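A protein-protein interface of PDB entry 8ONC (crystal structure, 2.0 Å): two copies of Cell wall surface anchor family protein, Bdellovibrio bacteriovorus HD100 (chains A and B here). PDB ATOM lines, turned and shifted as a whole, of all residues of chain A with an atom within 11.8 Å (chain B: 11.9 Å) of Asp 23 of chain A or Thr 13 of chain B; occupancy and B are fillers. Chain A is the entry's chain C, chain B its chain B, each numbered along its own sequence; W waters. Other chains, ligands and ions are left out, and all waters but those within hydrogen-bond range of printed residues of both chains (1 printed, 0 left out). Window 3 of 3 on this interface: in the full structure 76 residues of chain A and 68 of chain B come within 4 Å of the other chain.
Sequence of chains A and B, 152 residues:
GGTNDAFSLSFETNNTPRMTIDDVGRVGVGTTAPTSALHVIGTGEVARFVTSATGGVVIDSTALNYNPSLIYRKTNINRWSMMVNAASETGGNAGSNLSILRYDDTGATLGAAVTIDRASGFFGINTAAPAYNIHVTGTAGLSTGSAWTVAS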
ATOM      1  N   PHE A   7      11.467   2.878 -17.485  1.00  0.00           N
ATOM      2  CA  PHE A   7      10.578   3.780 -16.760  1.00  0.00           C
ATOM      3  C   PHE A   7      10.530   3.369 -15.288  1.00  0.00           C
ATOM      4  O   PHE A   7      10.146   2.245 -14.966  1.00  0.00           O
ATOM      5  CB  PHE A   7       9.176   3.775 -17.384  1.00  0.00           C
ATOM      6  CG  PHE A   7       9.155   4.123 -18.854  1.00  0.00           C
ATOM      7  CD1 PHE A   7       9.511   3.185 -19.815  1.00  0.00           C
ATOM      8  CD2 PHE A   7       8.786   5.391 -19.272  1.00  0.00           C
ATOM      9  CE1 PHE A   7       9.494   3.506 -21.162  1.00  0.00           C
ATOM     10  CE2 PHE A   7       8.768   5.718 -20.619  1.00  0.00           C
ATOM     11  CZ  PHE A   7       9.123   4.774 -21.564  1.00  0.00           C
ATOM     12  N   SER A   8      10.916   4.278 -14.394  1.00  0.00           N
ATOM     13  CA  SER A   8      11.160   3.909 -13.007  1.00  0.00           C
ATOM     14  C   SER A   8      10.923   5.100 -12.087  1.00  0.00           C
ATOM     15  O   SER A   8      10.851   6.251 -12.522  1.00  0.00           O
ATOM     16  CB  SER A   8      12.586   3.378 -12.826  1.00  0.00           C
ATOM     17  OG  SER A   8      13.541   4.381 -13.109  1.00  0.00           O
ATOM     18  N   LEU A   9      10.813   4.794 -10.798  1.00  0.00           N
ATOM     19  CA  LEU A   9      10.680   5.775  -9.728  1.00  0.00           C
ATOM     20  C   LEU A   9      11.929   5.742  -8.860  1.00  0.00           C
ATOM     21  O   LEU A   9      12.480   4.670  -8.598  1.00  0.00           O
ATOM     22  CB  LEU A   9       9.460   5.472  -8.855  1.00  0.00           C
ATOM     23  CG  LEU A   9       9.327   6.261  -7.544  1.00  0.00           C
ATOM     24  CD1 LEU A   9       9.223   7.779  -7.762  1.00  0.00           C
ATOM     25  CD2 LEU A   9       8.192   5.730  -6.686  1.00  0.00           C
ATOM     26  N   SER A  10      12.370   6.910  -8.396  1.00  0.00           N
ATOM     27  CA  SER A  10      13.514   6.998  -7.499  1.00  0.00           C
ATOM     28  C   SER A  10      13.155   7.788  -6.250  1.00  0.00           C
ATOM     29  O   SER A  10      12.477   8.817  -6.322  1.00  0.00           O
ATOM     30  CB  SER A  10      14.726   7.646  -8.184  1.00  0.00           C
ATOM     31  OG  SER A  10      15.267   6.794  -9.179  1.00  0.00           O
ATOM     32  N   MET A  19      17.237   4.896  -3.865  1.00  0.00           N
ATOM     33  CA  MET A  19      16.532   3.664  -4.178  1.00  0.00           C
ATOM     34  C   MET A  19      15.668   3.889  -5.408  1.00  0.00           C
ATOM     35  O   MET A  19      15.020   4.931  -5.541  1.00  0.00           O
ATOM     36  CB  MET A  19      15.669   3.194  -3.002  1.00  0.00           C
ATOM     37  CG  MET A  19      14.885   1.925  -3.285  1.00  0.00           C
ATOM     38  SD  MET A  19      13.799   1.468  -1.925  1.00  0.00           S
ATOM     39  CE  MET A  19      14.986   0.826  -0.760  1.00  0.00           C
ATOM     40  N   THR A  20      15.663   2.905  -6.302  1.00  0.00           N
ATOM     41  CA  THR A  20      14.948   2.988  -7.566  1.00  0.00           C
ATOM     42  C   THR A  20      14.110   1.734  -7.759  1.00  0.00           C
ATOM     43  O   THR A  20      14.582   0.622  -7.517  1.00  0.00           O
ATOM     44  CB  THR A  20      15.924   3.158  -8.740  1.00  0.00           C
ATOM     45  OG1 THR A  20      16.629   4.398  -8.603  1.00  0.00           O
ATOM     46  CG2 THR A  20      15.182   3.149 -10.072  1.00  0.00           C
ATOM     47  N   ILE A  21      12.861   1.916  -8.183  1.00  0.00           N
ATOM     48  CA  ILE A  21      11.955   0.813  -8.489  1.00  0.00           C
ATOM     49  C   ILE A  21      11.472   1.004  -9.918  1.00  0.00           C
ATOM     50  O   ILE A  21      10.870   2.037 -10.236  1.00  0.00           O
ATOM     51  CB  ILE A  21      10.766   0.759  -7.516  1.00  0.00           C
ATOM     52  CG1 ILE A  21      11.254   0.819  -6.067  1.00  0.00           C
ATOM     53  CG2 ILE A  21       9.942  -0.495  -7.751  1.00  0.00           C
ATOM     54  CD1 ILE A  21      10.250   1.416  -5.109  1.00  0.00           C
ATOM     55  N   ASP A  22      11.763   0.018 -10.761  1.00  0.00           N
ATOM     56  CA  ASP A  22      11.341   0.095 -12.181  1.00  0.00           C
ATOM     57  C   ASP A  22       9.996  -0.613 -12.390  1.00  0.00           C
ATOM     58  O   ASP A  22       9.530  -1.269 -11.468  1.00  0.00           O
ATOM     59  CB  ASP A  22      12.457  -0.371 -13.116  1.00  0.00           C
ATOM     60  CG  ASP A  22      12.789  -1.850 -13.056  1.00  0.00           C
ATOM     61  OD1 ASP A  22      11.938  -2.632 -12.610  1.00  0.00           O
ATOM     62  OD2 ASP A  22      13.901  -2.203 -13.477  1.00  0.00           O
ATOM     63  N   ASP A  23       9.428  -0.487 -13.585  1.00  0.00           N
ATOM     64  CA  ASP A  23       8.089  -1.062 -13.885  1.00  0.00           C
ATOM     65  C   ASP A  23       8.177  -2.571 -14.138  1.00  0.00           C
ATOM     66  O   ASP A  23       7.121  -3.196 -14.241  1.00  0.00           O
ATOM     67  CB  ASP A  23       7.427  -0.324 -15.052  1.00  0.00           C
ATOM     68  CG  ASP A  23       8.268  -0.234 -16.310  1.00  0.00           C
ATOM     69  OD1 ASP A  23       9.464  -0.555 -16.242  1.00  0.00           O
ATOM     70  OD2 ASP A  23       7.710   0.169 -17.345  1.00  0.00           O
ATOM     71  N   VAL A  24       9.383  -3.115 -14.255  1.00  0.00           N
ATOM     72  CA  VAL A  24       9.551  -4.586 -14.401  1.00  0.00           C
ATOM     73  C   VAL A  24       9.708  -5.176 -12.997  1.00  0.00           C
ATOM     74  O   VAL A  24       9.777  -6.401 -12.873  1.00  0.00           O
ATOM     75  CB  VAL A  24      10.735  -4.921 -15.327  1.00  0.00           C
ATOM     76  CG1 VAL A  24      10.878  -3.907 -16.449  1.00  0.00           C
ATOM     77  CG2 VAL A  24      12.042  -5.059 -14.565  1.00  0.00           C
ATOM     78  N   GLY A  25       9.795  -4.327 -11.978  1.00  0.00           N
ATOM     79  CA  GLY A  25       9.846  -4.841 -10.629  1.00  0.00           C
ATOM     80  C   GLY A  25      11.205  -4.928  -9.986  1.00  0.00           C
ATOM     81  O   GLY A  25      11.306  -5.454  -8.872  1.00  0.00           O
ATOM     82  N   ARG A  26      12.248  -4.425 -10.631  1.00  0.00           N
ATOM     83  CA  ARG A  26      13.589  -4.504 -10.078  1.00  0.00           C
ATOM     84  C   ARG A  26      13.846  -3.314  -9.166  1.00  0.00           C
ATOM     85  O   ARG A  26      13.444  -2.186  -9.466  1.00  0.00           O
ATOM     86  CB  ARG A  26      14.622  -4.559 -11.200  1.00  0.00           C
ATOM     87  CG  ARG A  26      14.656  -5.906 -11.888  1.00  0.00           C
ATOM     88  CD  ARG A  26      15.695  -5.938 -12.984  1.00  0.00           C
ATOM     89  NE  ARG A  26      15.392  -4.976 -14.035  1.00  0.00           N
ATOM     90  CZ  ARG A  26      15.670  -5.163 -15.317  1.00  0.00           C
ATOM     91  NH1 ARG A  26      16.255  -6.271 -15.743  1.00  0.00           N
ATOM     92  NH2 ARG A  26      15.349  -4.217 -16.194  1.00  0.00           N
ATOM     93  N   VAL A  27      14.500  -3.580  -8.040  1.00  0.00           N
ATOM     94  CA  VAL A  27      14.796  -2.572  -7.034  1.00  0.00           C
ATOM     95  C   VAL A  27      16.305  -2.414  -6.949  1.00  0.00           C
ATOM     96  O   VAL A  27      17.030  -3.401  -6.772  1.00  0.00           O
ATOM     97  CB  VAL A  27      14.203  -2.950  -5.665  1.00  0.00           C
ATOM     98  CG1 VAL A  27      14.588  -1.922  -4.613  1.00  0.00           C
ATOM     99  CG2 VAL A  27      12.694  -3.080  -5.773  1.00  0.00           C
ATOM    100  N   GLY A  28      16.772  -1.182  -7.090  1.00  0.00           N
ATOM    101  CA  GLY A  28      18.184  -0.858  -6.989  1.00  0.00           C
ATOM    102  C   GLY A  28      18.434   0.044  -5.792  1.00  0.00           C
ATOM    103  O   GLY A  28      17.687   0.998  -5.559  1.00  0.00           O
ATOM    104  N   THR A  31      21.931   2.167  -7.310  1.00  0.00           N
ATOM    105  CA  THR A  31      21.905   2.196  -8.765  1.00  0.00           C
ATOM    106  C   THR A  31      20.522   2.601  -9.241  1.00  0.00           C
ATOM    107  O   THR A  31      19.511   2.196  -8.658  1.00  0.00           O
ATOM    108  CB  THR A  31      22.266   0.841  -9.388  1.00  0.00           C
ATOM    109  OG1 THR A  31      22.053   0.893 -10.801  1.00  0.00           O
ATOM    110  CG2 THR A  31      21.416  -0.277  -8.800  1.00  0.00           C
ATOM    111  N   THR A  32      20.483   3.403 -10.297  1.00  0.00           N
ATOM    112  CA  THR A  32      19.239   3.693 -10.993  1.00  0.00           C
ATOM    113  C   THR A  32      18.973   2.717 -12.129  1.00  0.00           C
ATOM    114  O   THR A  32      17.945   2.836 -12.804  1.00  0.00           O
ATOM    115  CB  THR A  32      19.250   5.126 -11.530  1.00  0.00           C
ATOM    116  OG1 THR A  32      20.363   5.295 -12.416  1.00  0.00           O
ATOM    117  CG2 THR A  32      19.364   6.119 -10.386  1.00  0.00           C
ATOM    118  N   ALA A  33      19.867   1.755 -12.354  1.00  0.00           N
ATOM    119  CA  ALA A  33      19.707   0.748 -13.403  1.00  0.00           C
ATOM    120  C   ALA A  33      19.906  -0.644 -12.814  1.00  0.00           C
ATOM    121  O   ALA A  33      20.896  -1.323 -13.112  1.00  0.00           O
ATOM    122  CB  ALA A  33      20.685   1.002 -14.552  1.00  0.00           C
ATOM    123  N   PRO A  34      18.976  -1.105 -11.977  1.00  0.00           N
ATOM    124  CA  PRO A  34      19.117  -2.448 -11.400  1.00  0.00           C
ATOM    125  C   PRO A  34      18.973  -3.523 -12.465  1.00  0.00           C
ATOM    126  O   PRO A  34      18.130  -3.429 -13.360  1.00  0.00           O
ATOM    127  CB  PRO A  34      17.977  -2.518 -10.376  1.00  0.00           C
ATOM    128  CG  PRO A  34      16.968  -1.537 -10.879  1.00  0.00           C
ATOM    129  CD  PRO A  34      17.763  -0.423 -11.491  1.00  0.00           C
ATOM    130  N   THR A  35      19.807  -4.555 -12.359  1.00  0.00           N
ATOM    131  CA  THR A  35      19.787  -5.670 -13.296  1.00  0.00           C
ATOM    132  C   THR A  35      19.239  -6.952 -12.687  1.00  0.00           C
ATOM    133  O   THR A  35      19.256  -7.994 -13.350  1.00  0.00           O
ATOM    134  CB  THR A  35      21.192  -5.919 -13.851  1.00  0.00           C
ATOM    135  OG1 THR A  35      22.074  -6.274 -12.776  1.00  0.00           O
ATOM    136  CG2 THR A  35      21.718  -4.668 -14.543  1.00  0.00           C
ATOM    137  N   SER A  36      18.763  -6.905 -11.445  1.00  0.00           N
ATOM    138  CA  SER A  36      18.140  -8.047 -10.792  1.00  0.00           C
ATOM    139  C   SER A  36      17.018  -7.534  -9.900  1.00  0.00           C
ATOM    140  O   SER A  36      16.877  -6.326  -9.687  1.00  0.00           O
ATOM    141  CB  SER A  36      19.161  -8.859  -9.986  1.00  0.00           C
ATOM    142  OG  SER A  36      19.778  -8.065  -8.990  1.00  0.00           O
ATOM    143  N   ALA A  37      16.214  -8.467  -9.377  1.00  0.00           N
ATOM    144  CA  ALA A  37      15.071  -8.083  -8.548  1.00  0.00           C
ATOM    145  C   ALA A  37      15.501  -7.204  -7.380  1.00  0.00           C
ATOM    146  O   ALA A  37      14.790  -6.265  -7.004  1.00  0.00           O
ATOM    147  CB  ALA A  37      14.339  -9.328  -8.047  1.00  0.00           C
ATOM    148  N   LEU B   9       3.370  -0.195  -3.753  1.00  0.00           N
ATOM    149  CA  LEU B   9       3.739   0.744  -4.804  1.00  0.00           C
ATOM    150  C   LEU B   9       3.531   0.066  -6.149  1.00  0.00           C
ATOM    151  O   LEU B   9       4.094  -1.004  -6.389  1.00  0.00           O
ATOM    152  CB  LEU B   9       5.203   1.167  -4.666  1.00  0.00           C
ATOM    153  CG  LEU B   9       5.637   1.756  -3.327  1.00  0.00           C
ATOM    154  CD1 LEU B   9       7.145   1.703  -3.178  1.00  0.00           C
ATOM    155  CD2 LEU B   9       5.156   3.174  -3.238  1.00  0.00           C
ATOM    156  N   SER B  10       2.723   0.668  -7.016  1.00  0.00           N
ATOM    157  CA  SER B  10       2.426   0.076  -8.343  1.00  0.00           C
ATOM    158  C   SER B  10       2.659   1.084  -9.467  1.00  0.00           C
ATOM    159  O   SER B  10       2.721   2.287  -9.182  1.00  0.00           O
ATOM    160  CB  SER B  10       1.034  -0.455  -8.401  1.00  0.00           C
ATOM    161  OG  SER B  10       0.696  -1.117  -7.194  1.00  0.00           O
ATOM    162  N   PHE B  11       2.800   0.586 -10.690  1.00  0.00           N
ATOM    163  CA  PHE B  11       2.975   1.466 -11.868  1.00  0.00           C
ATOM    164  C   PHE B  11       1.751   1.309 -12.782  1.00  0.00           C
ATOM    165  O   PHE B  11       1.267   0.190 -12.971  1.00  0.00           O
ATOM    166  CB  PHE B  11       4.312   1.169 -12.544  1.00  0.00           C
ATOM    167  CG  PHE B  11       5.533   1.587 -11.770  1.00  0.00           C
ATOM    168  CD1 PHE B  11       5.921   2.914 -11.716  1.00  0.00           C
ATOM    169  CD2 PHE B  11       6.307   0.648 -11.110  1.00  0.00           C
ATOM    170  CE1 PHE B  11       7.048   3.293 -11.009  1.00  0.00           C
ATOM    171  CE2 PHE B  11       7.436   1.030 -10.404  1.00  0.00           C
ATOM    172  CZ  PHE B  11       7.803   2.349 -10.353  1.00  0.00           C
ATOM    173  N   GLU B  12       1.233   2.420 -13.303  1.00  0.00           N
ATOM    174  CA  GLU B  12       0.003   2.380 -14.144  1.00  0.00           C
ATOM    175  C   GLU B  12       0.355   1.695 -15.468  1.00  0.00           C
ATOM    176  O   GLU B  12      -0.573   1.337 -16.199  1.00  0.00           O
ATOM    177  CB  GLU B  12      -0.573   3.785 -14.324  1.00  0.00           C
ATOM    178  CG  GLU B  12      -2.040   3.815 -14.715  1.00  0.00           C
ATOM    179  CD  GLU B  12      -2.994   3.068 -13.795  1.00  0.00           C
ATOM    180  OE1 GLU B  12      -2.946   3.302 -12.573  1.00  0.00           O
ATOM    181  OE2 GLU B  12      -3.807   2.280 -14.312  1.00  0.00           O
ATOM    182  N   THR B  13       1.651   1.477 -15.718  1.00  0.00           N
ATOM    183  CA  THR B  13       2.100   0.758 -16.937  1.00  0.00           C
ATOM    184  C   THR B  13       1.607  -0.693 -16.931  1.00  0.00           C
ATOM    185  O   THR B  13       1.118  -1.138 -17.984  1.00  0.00           O
ATOM    186  CB  THR B  13       3.626   0.775 -17.034  1.00  0.00           C
ATOM    187  OG1 THR B  13       4.105  -0.023 -15.952  1.00  0.00           O
ATOM    188  CG2 THR B  13       4.210   2.168 -16.959  1.00  0.00           C
ATOM    189  N   ASN B  14       1.714  -1.390 -15.796  1.00  0.00           N
ATOM    190  CA  ASN B  14       1.304  -2.815 -15.698  1.00  0.00           C
ATOM    191  C   ASN B  14       0.290  -2.994 -14.570  1.00  0.00           C
ATOM    192  O   ASN B  14      -0.305  -4.079 -14.484  1.00  0.00           O
ATOM    193  CB  ASN B  14       2.509  -3.717 -15.438  1.00  0.00           C
ATOM    194  CG  ASN B  14       3.645  -3.494 -16.411  1.00  0.00           C
ATOM    195  OD1 ASN B  14       3.484  -3.678 -17.616  1.00  0.00           O
ATOM    196  ND2 ASN B  14       4.797  -3.099 -15.898  1.00  0.00           N
ATOM    197  N   ASN B  15       0.133  -1.985 -13.719  1.00  0.00           N
ATOM    198  CA  ASN B  15      -0.841  -2.052 -12.596  1.00  0.00           C
ATOM    199  C   ASN B  15      -0.379  -3.089 -11.570  1.00  0.00           C
ATOM    200  O   ASN B  15      -1.130  -3.350 -10.615  1.00  0.00           O
ATOM    201  CB  ASN B  15      -2.255  -2.367 -13.085  1.00  0.00           C
ATOM    202  CG  ASN B  15      -2.838  -1.238 -13.907  1.00  0.00           C
ATOM    203  OD1 ASN B  15      -2.917  -0.105 -13.441  1.00  0.00           O
ATOM    204  ND2 ASN B  15      -3.233  -1.532 -15.134  1.00  0.00           N
ATOM    205  N   THR B  16       0.822  -3.631 -11.751  1.00  0.00           N
ATOM    206  CA  THR B  16       1.307  -4.695 -10.837  1.00  0.00           C
ATOM    207  C   THR B  16       2.048  -4.086  -9.644  1.00  0.00           C
ATOM    208  O   THR B  16       2.865  -3.184  -9.859  1.00  0.00           O
ATOM    209  CB  THR B  16       2.171  -5.697 -11.606  1.00  0.00           C
ATOM    210  OG1 THR B  16       3.177  -4.913 -12.244  1.00  0.00           O
ATOM    211  CG2 THR B  16       1.396  -6.480 -12.639  1.00  0.00           C
ATOM    212  N   PRO B  17       1.749  -4.515  -8.401  1.00  0.00           N
ATOM    213  CA  PRO B  17       2.515  -4.076  -7.225  1.00  0.00           C
ATOM    214  C   PRO B  17       3.955  -4.564  -7.308  1.00  0.00           C
ATOM    215  O   PRO B  17       4.219  -5.731  -7.603  1.00  0.00           O
ATOM    216  CB  PRO B  17       1.770  -4.707  -6.043  1.00  0.00           C
ATOM    217  CG  PRO B  17       0.883  -5.745  -6.619  1.00  0.00           C
ATOM    218  CD  PRO B  17       0.682  -5.474  -8.070  1.00  0.00           C
ATOM    219  N   ARG B  18       4.885  -3.653  -7.036  1.00  0.00           N
ATOM    220  CA  ARG B  18       6.313  -3.890  -7.163  1.00  0.00           C
ATOM    221  C   ARG B  18       7.031  -3.976  -5.829  1.00  0.00           C
ATOM    222  O   ARG B  18       8.005  -4.723  -5.711  1.00  0.00           O
ATOM    223  CB  ARG B  18       6.942  -2.774  -8.003  1.00  0.00           C
ATOM    224  CG  ARG B  18       6.381  -2.738  -9.407  1.00  0.00           C
ATOM    225  CD  ARG B  18       6.733  -4.038 -10.075  1.00  0.00           C
ATOM    226  NE  ARG B  18       6.135  -4.244 -11.386  1.00  0.00           N
ATOM    227  CZ  ARG B  18       6.009  -5.436 -11.955  1.00  0.00           C
ATOM    228  NH1 ARG B  18       6.420  -6.538 -11.346  1.00  0.00           N
ATOM    229  NH2 ARG B  18       5.475  -5.523 -13.168  1.00  0.00           N
ATOM    230  N   MET B  19       6.576  -3.227  -4.830  1.00  0.00           N
ATOM    231  CA  MET B  19       7.090  -3.310  -3.473  1.00  0.00           C
ATOM    232  C   MET B  19       5.919  -3.229  -2.509  1.00  0.00           C
ATOM    233  O   MET B  19       4.969  -2.474  -2.736  1.00  0.00           O
ATOM    234  CB  MET B  19       8.090  -2.191  -3.171  1.00  0.00           C
ATOM    235  CG  MET B  19       8.845  -2.377  -1.865  1.00  0.00           C
ATOM    236  SD  MET B  19      10.113  -1.123  -1.619  1.00  0.00           S
ATOM    237  CE  MET B  19      11.406  -1.746  -2.687  1.00  0.00           C
ATOM    238  N   VAL B  29       9.476  -7.713  -2.284  1.00  0.00           N
ATOM    239  CA  VAL B  29       9.852  -7.257  -3.617  1.00  0.00           C
ATOM    240  C   VAL B  29       9.438  -8.354  -4.585  1.00  0.00           C
ATOM    241  O   VAL B  29      10.086  -9.406  -4.655  1.00  0.00           O
ATOM    242  CB  VAL B  29      11.351  -6.957  -3.728  1.00  0.00           C
ATOM    243  CG1 VAL B  29      11.694  -6.524  -5.142  1.00  0.00           C
ATOM    244  CG2 VAL B  29      11.751  -5.884  -2.727  1.00  0.00           C
ATOM    245  N   GLY B  30       8.361  -8.117  -5.325  1.00  0.00           N
ATOM    246  CA  GLY B  30       7.799  -9.134  -6.183  1.00  0.00           C
ATOM    247  C   GLY B  30       6.752 -10.005  -5.528  1.00  0.00           C
ATOM    248  O   GLY B  30       6.190 -10.880  -6.200  1.00  0.00           O
ATOM    249  N   ILE B  41      11.535 -11.984  -4.767  1.00  0.00           N
ATOM    250  CA  ILE B  41      11.285 -13.020  -5.763  1.00  0.00           C
ATOM    251  C   ILE B  41      11.783 -12.544  -7.119  1.00  0.00           C
ATOM    252  O   ILE B  41      11.563 -11.391  -7.505  1.00  0.00           O
ATOM    253  CB  ILE B  41       9.793 -13.411  -5.829  1.00  0.00           C
ATOM    254  CG1 ILE B  41       9.383 -14.126  -4.546  1.00  0.00           C
ATOM    255  CG2 ILE B  41       9.501 -14.283  -7.035  1.00  0.00           C
ATOM    256  CD1 ILE B  41       7.978 -13.863  -4.154  1.00  0.00           C
HETATM  257  O   HOH W   1       9.148  -5.742  -7.754  1.00  0.00           O
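The side-chain amide nitrogen of Asn 14 of chain B sits at hydrogen-bond distance from the backbone carbonyl oxygen of Asp 23 of chain A (2.9 Å). NH2 of Arg 18 of chain B lies within hydrogen-bond range of O of Asp 23 of chain A, 3.0 Å away.
N of Val 27 of chain A is in hydrogen-bond range of O of Ala 37 of chain A (2.9 Å). OG1 of Thr 16 of chain B is in hydrogen-bond range of NH2 of Arg 18 of chain B, 2.6 Å away. The backbone carbonyl oxygen of Arg 18 of chain B is in hydrogen-bond range of the backbone NH of Gly 30 of chain B. The side-chain carboxylate (OD1) of Asp 22 of chain A lies within hydrogen-bond range of the backbone NH (N) of Gly 25 of chain A, at 2.8 Å. O of Leu 9 of chain A lies within hydrogen-bond range of N of Ile 21 of chain A. The backbone NH (N) of Ile 41 of chain B lies within hydrogen-bond range of the backbone carbonyl oxygen (O) of Val 29 of chain B, 3.0 Å away.
Among the printed residues, merely in contact across the chains: Leu 9 of chain A with Phe 11 of chain B (3.8 Å), Ile 21 of chain A with Leu 9 of chain B (3.7 Å), Ile 21 of chain A with Phe 11 of chain B (3.1 Å), Ile 21 of chain A with Arg 18 of chain B (3.8 Å), Asp 22 of chain A with Phe 11 of chain B (3.3 Å), Asp 23 of chain A with Phe 11 of chain B (3.7 Å), Asp 23 of chain A with Thr 13 of chain B (3.5 Å), Val 24 of chain A with Arg 18 of chain B (3.7 Å), Gly 25 of chain A with Arg 18 of chain B (3.3 Å), Gly 25 of chain A with Val 29 of chain B (3.9 Å), Val 27 of chain A with Met 19 of chain B (3.6 Å), Val 27 of chain A with Val 29 of chain B (3.6 Å), Ala 37 of chain A with Val 29 of chain B (3.6 Å) and Ala 37 of chain A with Ile 41 of chain B (3.5 Å).
No residue of chain B comes within 4 Å of Phe 7 of chain A. No residue of chain B comes within 4 Å of Ser 8 of chain A. Of the printed residues of chain B, Leu 9 of chain A touches Phe 11 (3.8 Å). Asp 22 of chain A touches just one residue of chain B: Phe 11 (3.3 Å). Of chain B, only Phe 11 (3.7 Å), Thr 13 (3.5 Å), Asn 14 (2.9 Å) and Arg 18 (3.0 Å) come within 4 Å of Asp 23 of chain A. Printed residues of chain B within 4 Å of Val 27 of chain A: Met 19 and Val 29. Thr 35 of chain A touches none of the printed residues of chain B. Printed residues of chain B within 4 Å of Ala 37 of chain A: Val 29 (3.6 Å) and Ile 41 (3.5 Å). Of the printed residues of chain A, Leu 9 of chain B touches Ile 21. No residue of chain A comes within 4 Å of Glu 12 of chain B. Of the printed residues of chain A, Thr 13 of chain B touches Asp 23. Asn 14 of chain B touches one residue of chain A. Asn 15 of chain B touches none of the printed residues of chain A. Of the printed residues of chain A, Met 19 of chain B touches Val 27. The nearest residue of chain B that does not touch Asp 23 of chain A is Thr 16 of chain B (4.7 Å).
Of the 21 printed residues of chain A, 8 touch a printed residue of chain B. Hydrophobic or aromatic side chains of chain A that line the printed part of chain B: Leu 9, Ile 21, Val 27 and Ala 37. Along chain A the printed residues that touch a printed residue of chain B span positions 9 to 37. Of the 14 printed residues of chain B, 8 touch a printed residue of chain A. Among the printed residues, no Asp or Glu carboxylate lies within 4 Å of a Lys or Arg side-chain nitrogen of the other chain.
Positions printed for both chains: 9, 10 and 19. Of the 16 pairs that touch across the chains among the printed residues, none has its exchanged pair printed and touching as well.
Water W1 lies within hydrogen-bond range of the backbone carbonyl oxygen of Gly 25 of chain A (2.4 Å), the backbone carbonyl oxygen of Arg 18 of chain B (2.6 Å) and the backbone NH of Gly 30 of chain B (3.5 Å).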
